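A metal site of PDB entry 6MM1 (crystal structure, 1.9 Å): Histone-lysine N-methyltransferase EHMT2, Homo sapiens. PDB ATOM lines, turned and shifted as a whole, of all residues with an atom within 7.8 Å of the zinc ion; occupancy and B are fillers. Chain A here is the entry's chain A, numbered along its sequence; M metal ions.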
ATOM      1  N   SER A  35       8.290   0.793  -6.194  1.00  0.00           N
ATOM      2  CA  SER A  35       7.683  -0.530  -6.119  1.00  0.00           C
ATOM      3  C   SER A  35       8.541  -1.431  -5.237  1.00  0.00           C
ATOM      4  O   SER A  35       9.745  -1.540  -5.444  1.00  0.00           O
ATOM      5  CB  SER A  35       7.544  -1.146  -7.516  1.00  0.00           C
ATOM      6  OG  SER A  35       6.906  -2.417  -7.452  1.00  0.00           O
ATOM      7  N   CYS A  77      15.240   2.471 -12.369  1.00  0.00           N
ATOM      8  CA  CYS A  77      13.819   2.544 -12.650  1.00  0.00           C
ATOM      9  C   CYS A  77      13.488   1.541 -13.747  1.00  0.00           C
ATOM     10  O   CYS A  77      14.227   1.399 -14.722  1.00  0.00           O
ATOM     11  CB  CYS A  77      13.432   3.959 -13.091  1.00  0.00           C
ATOM     12  SG  CYS A  77      11.646   4.220 -13.151  1.00  0.00           S
ATOM     13  N   CYS A  78      12.379   0.825 -13.584  1.00  0.00           N
ATOM     14  CA  CYS A  78      12.037  -0.230 -14.543  1.00  0.00           C
ATOM     15  C   CYS A  78      11.476   0.367 -15.832  1.00  0.00           C
ATOM     16  O   CYS A  78      10.452   1.059 -15.786  1.00  0.00           O
ATOM     17  CB  CYS A  78      11.030  -1.206 -13.939  1.00  0.00           C
ATOM     18  SG  CYS A  78      10.734  -2.612 -15.013  1.00  0.00           S
ATOM     19  N   PRO A  79      12.078   0.089 -16.990  1.00  0.00           N
ATOM     20  CA  PRO A  79      11.508   0.598 -18.244  1.00  0.00           C
ATOM     21  C   PRO A  79      10.184  -0.037 -18.593  1.00  0.00           C
ATOM     22  O   PRO A  79       9.453   0.520 -19.429  1.00  0.00           O
ATOM     23  CB  PRO A  79      12.584   0.241 -19.294  1.00  0.00           C
ATOM     24  CG  PRO A  79      13.816  -0.119 -18.504  1.00  0.00           C
ATOM     25  CD  PRO A  79      13.306  -0.679 -17.209  1.00  0.00           C
ATOM     26  N   GLY A  80       9.826  -1.173 -17.997  1.00  0.00           N
ATOM     27  CA  GLY A  80       8.610  -1.857 -18.388  1.00  0.00           C
ATOM     28  C   GLY A  80       7.397  -1.193 -17.810  1.00  0.00           C
ATOM     29  O   GLY A  80       6.401  -0.966 -18.510  1.00  0.00           O
ATOM     30  N   CYS A  81       7.455  -0.842 -16.515  1.00  0.00           N
ATOM     31  CA  CYS A  81       6.317  -0.269 -15.813  1.00  0.00           C
ATOM     32  C   CYS A  81       6.541   1.164 -15.360  1.00  0.00           C
ATOM     33  O   CYS A  81       5.568   1.869 -15.066  1.00  0.00           O
ATOM     34  CB  CYS A  81       5.978  -1.124 -14.586  1.00  0.00           C
ATOM     35  SG  CYS A  81       7.371  -1.403 -13.442  1.00  0.00           S
ATOM     36  N   GLY A  82       7.781   1.623 -15.311  1.00  0.00           N
ATOM     37  CA  GLY A  82       8.066   2.954 -14.837  1.00  0.00           C
ATOM     38  C   GLY A  82       8.184   3.109 -13.345  1.00  0.00           C
ATOM     39  O   GLY A  82       8.261   4.239 -12.854  1.00  0.00           O
ATOM     40  N   TYR A  83       8.207   2.014 -12.595  1.00  0.00           N
ATOM     41  CA  TYR A  83       8.394   2.071 -11.151  1.00  0.00           C
ATOM     42  C   TYR A  83       9.850   1.867 -10.782  1.00  0.00           C
ATOM     43  O   TYR A  83      10.570   1.093 -11.419  1.00  0.00           O
ATOM     44  CB  TYR A  83       7.541   1.015 -10.444  1.00  0.00           C
ATOM     45  CG  TYR A  83       6.066   1.089 -10.772  1.00  0.00           C
ATOM     46  CD1 TYR A  83       5.447   2.302 -11.027  1.00  0.00           C
ATOM     47  CD2 TYR A  83       5.287  -0.061 -10.837  1.00  0.00           C
ATOM     48  CE1 TYR A  83       4.101   2.375 -11.341  1.00  0.00           C
ATOM     49  CE2 TYR A  83       3.944  -0.010 -11.152  1.00  0.00           C
ATOM     50  CZ  TYR A  83       3.355   1.210 -11.403  1.00  0.00           C
ATOM     51  OH  TYR A  83       2.009   1.282 -11.707  1.00  0.00           O
ATOM     52  N   PHE A  84      10.275   2.539  -9.713  1.00  0.00           N
ATOM     53  CA  PHE A  84      11.639   2.398  -9.229  1.00  0.00           C
ATOM     54  C   PHE A  84      11.808   1.087  -8.474  1.00  0.00           C
ATOM     55  O   PHE A  84      10.939   0.685  -7.694  1.00  0.00           O
ATOM     56  CB  PHE A  84      12.013   3.567  -8.330  1.00  0.00           C
ATOM     57  CG  PHE A  84      12.381   4.801  -9.091  1.00  0.00           C
ATOM     58  CD1 PHE A  84      11.406   5.658  -9.545  1.00  0.00           C
ATOM     59  CD2 PHE A  84      13.721   5.094  -9.353  1.00  0.00           C
ATOM     60  CE1 PHE A  84      11.748   6.806 -10.242  1.00  0.00           C
ATOM     61  CE2 PHE A  84      14.068   6.233 -10.050  1.00  0.00           C
ATOM     62  CZ  PHE A  84      13.079   7.093 -10.495  1.00  0.00           C
ATOM     63  N   CYS A  85      12.937   0.422  -8.699  1.00  0.00           N
ATOM     64  CA  CYS A  85      13.291  -0.796  -7.980  1.00  0.00           C
ATOM     65  C   CYS A  85      14.314  -0.411  -6.921  1.00  0.00           C
ATOM     66  O   CYS A  85      15.522  -0.483  -7.146  1.00  0.00           O
ATOM     67  CB  CYS A  85      13.860  -1.847  -8.921  1.00  0.00           C
ATOM     68  SG  CYS A  85      12.906  -2.184 -10.422  1.00  0.00           S
ATOM     69  N   ARG A 102      18.206  -2.471 -13.295  1.00  0.00           N
ATOM     70  CA  ARG A 102      17.203  -3.122 -12.482  1.00  0.00           C
ATOM     71  C   ARG A 102      15.892  -3.176 -13.232  1.00  0.00           C
ATOM     72  O   ARG A 102      15.503  -2.215 -13.908  1.00  0.00           O
ATOM     73  CB  ARG A 102      17.001  -2.403 -11.146  1.00  0.00           C
ATOM     74  CG  ARG A 102      18.242  -2.297 -10.300  1.00  0.00           C
ATOM     75  CD  ARG A 102      17.929  -1.670  -8.951  1.00  0.00           C
ATOM     76  NE  ARG A 102      19.075  -1.764  -8.056  1.00  0.00           N
ATOM     77  CZ  ARG A 102      19.130  -1.216  -6.852  1.00  0.00           C
ATOM     78  NH1 ARG A 102      18.106  -0.505  -6.392  1.00  0.00           N
ATOM     79  NH2 ARG A 102      20.230  -1.353  -6.115  1.00  0.00           N
ATOM     80  N   PHE A 103      15.181  -4.292 -13.087  1.00  0.00           N
ATOM     81  CA  PHE A 103      13.892  -4.438 -13.749  1.00  0.00           C
ATOM     82  C   PHE A 103      13.137  -5.597 -13.107  1.00  0.00           C
ATOM     83  O   PHE A 103      13.724  -6.423 -12.412  1.00  0.00           O
ATOM     84  CB  PHE A 103      14.061  -4.650 -15.253  1.00  0.00           C
ATOM     85  CG  PHE A 103      15.012  -5.758 -15.621  1.00  0.00           C
ATOM     86  CD1 PHE A 103      16.376  -5.554 -15.653  1.00  0.00           C
ATOM     87  CD2 PHE A 103      14.527  -7.012 -15.952  1.00  0.00           C
ATOM     88  CE1 PHE A 103      17.243  -6.573 -15.985  1.00  0.00           C
ATOM     89  CE2 PHE A 103      15.388  -8.036 -16.305  1.00  0.00           C
ATOM     90  CZ  PHE A 103      16.751  -7.819 -16.307  1.00  0.00           C
ATOM     91  N   HIS A 104      11.828  -5.619 -13.341  1.00  0.00           N
ATOM     92  CA  HIS A 104      10.989  -6.716 -12.887  1.00  0.00           C
ATOM     93  C   HIS A 104      11.035  -7.870 -13.870  1.00  0.00           C
ATOM     94  O   HIS A 104      11.124  -7.680 -15.089  1.00  0.00           O
ATOM     95  CB  HIS A 104       9.551  -6.222 -12.735  1.00  0.00           C
ATOM     96  CG  HIS A 104       9.390  -5.209 -11.651  1.00  0.00           C
ATOM     97  ND1 HIS A 104       9.653  -3.878 -11.854  1.00  0.00           N
ATOM     98  CD2 HIS A 104       8.927  -5.326 -10.388  1.00  0.00           C
ATOM     99  CE1 HIS A 104       9.400  -3.218 -10.738  1.00  0.00           C
ATOM    100  NE2 HIS A 104       8.954  -4.074  -9.835  1.00  0.00           N
ATOM    101  N   LYS A 105      10.953  -9.093 -13.329  1.00  0.00           N
ATOM    102  CA  LYS A 105      10.925 -10.270 -14.201  1.00  0.00           C
ATOM    103  C   LYS A 105       9.850 -10.133 -15.277  1.00  0.00           C
ATOM    104  O   LYS A 105      10.078 -10.480 -16.439  1.00  0.00           O
ATOM    105  CB  LYS A 105      10.688 -11.538 -13.367  1.00  0.00           C
ATOM    106  CG  LYS A 105      10.941 -12.831 -14.113  1.00  0.00           C
ATOM    107  CD  LYS A 105       9.662 -13.382 -14.735  1.00  0.00           C
ATOM    108  CE  LYS A 105       9.867 -14.773 -15.300  1.00  0.00           C
ATOM    109  NZ  LYS A 105      10.227 -15.771 -14.256  1.00  0.00           N
ATOM    110  N   ALA A 106       8.691  -9.603 -14.912  1.00  0.00           N
ATOM    111  CA  ALA A 106       7.590  -9.470 -15.871  1.00  0.00           C
ATOM    112  C   ALA A 106       7.810  -8.344 -16.875  1.00  0.00           C
ATOM    113  O   ALA A 106       7.051  -8.244 -17.839  1.00  0.00           O
ATOM    114  CB  ALA A 106       6.275  -9.232 -15.125  1.00  0.00           C
ATOM    115  N   CYS A 107       8.825  -7.504 -16.680  1.00  0.00           N
ATOM    116  CA  CYS A 107       9.017  -6.334 -17.513  1.00  0.00           C
ATOM    117  C   CYS A 107      10.202  -6.491 -18.460  1.00  0.00           C
ATOM    118  O   CYS A 107      10.679  -5.493 -19.030  1.00  0.00           O
ATOM    119  CB  CYS A 107       9.171  -5.092 -16.645  1.00  0.00           C
ATOM    120  SG  CYS A 107       7.717  -4.711 -15.554  1.00  0.00           S
ATOM    121  N   VAL A 108      10.680  -7.717 -18.665  1.00  0.00           N
ATOM    122  CA  VAL A 108      11.763  -7.938 -19.606  1.00  0.00           C
ATOM    123  C   VAL A 108      11.283  -7.611 -21.021  1.00  0.00           C
ATOM    124  O   VAL A 108      10.084  -7.682 -21.317  1.00  0.00           O
ATOM    125  CB  VAL A 108      12.272  -9.388 -19.537  1.00  0.00           C
ATOM    126  CG1 VAL A 108      12.885  -9.668 -18.176  1.00  0.00           C
ATOM    127  CG2 VAL A 108      11.139 -10.374 -19.844  1.00  0.00           C
ATOM    128  N   PRO A 118      15.566  -4.835 -20.417  1.00  0.00           N
ATOM    129  CA  PRO A 118      14.885  -3.701 -21.056  1.00  0.00           C
ATOM    130  C   PRO A 118      15.677  -2.414 -21.022  1.00  0.00           C
ATOM    131  O   PRO A 118      15.205  -1.408 -21.564  1.00  0.00           O
ATOM    132  CB  PRO A 118      13.592  -3.567 -20.253  1.00  0.00           C
ATOM    133  CG  PRO A 118      13.964  -4.045 -18.918  1.00  0.00           C
ATOM    134  CD  PRO A 118      14.985  -5.155 -19.097  1.00  0.00           C
HETATM  135 ZN    ZN M   1       8.635  -3.170 -14.103  1.00  0.00          ZN
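The zinc ion is bound by the side-chain sulfur of Cys 81 (2.3 Å), the side-chain sulfur of Cys 107 (2.3 Å), the side-chain sulfur of Cys 78 (2.4 Å) and a ring nitrogen (ND1) of His 104 (2.6 Å). The zinc ion has four donor atoms within binding distance.
The backbone NH of Tyr 83 lies close to the side-chain sulfur of Cys 81 (3.6 Å). The backbone NH (N) of Gly 80 lies close to the side-chain sulfur (SG) of Cys 78, 3.4 Å away. The backbone carbonyl oxygen (O) of Tyr 83 sits at hydrogen-bond distance from the backbone NH (N) of Cys 78 (2.8 Å).
Within 4 Å of the zinc ion: Cys 78, Cys 81, His 104 and Cys 107. Along chain A the residues within 4 Å of the zinc ion span positions 78 to 107. The nearest printed residue that does not touch the zinc ion is Gly 80 (4.4 Å).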
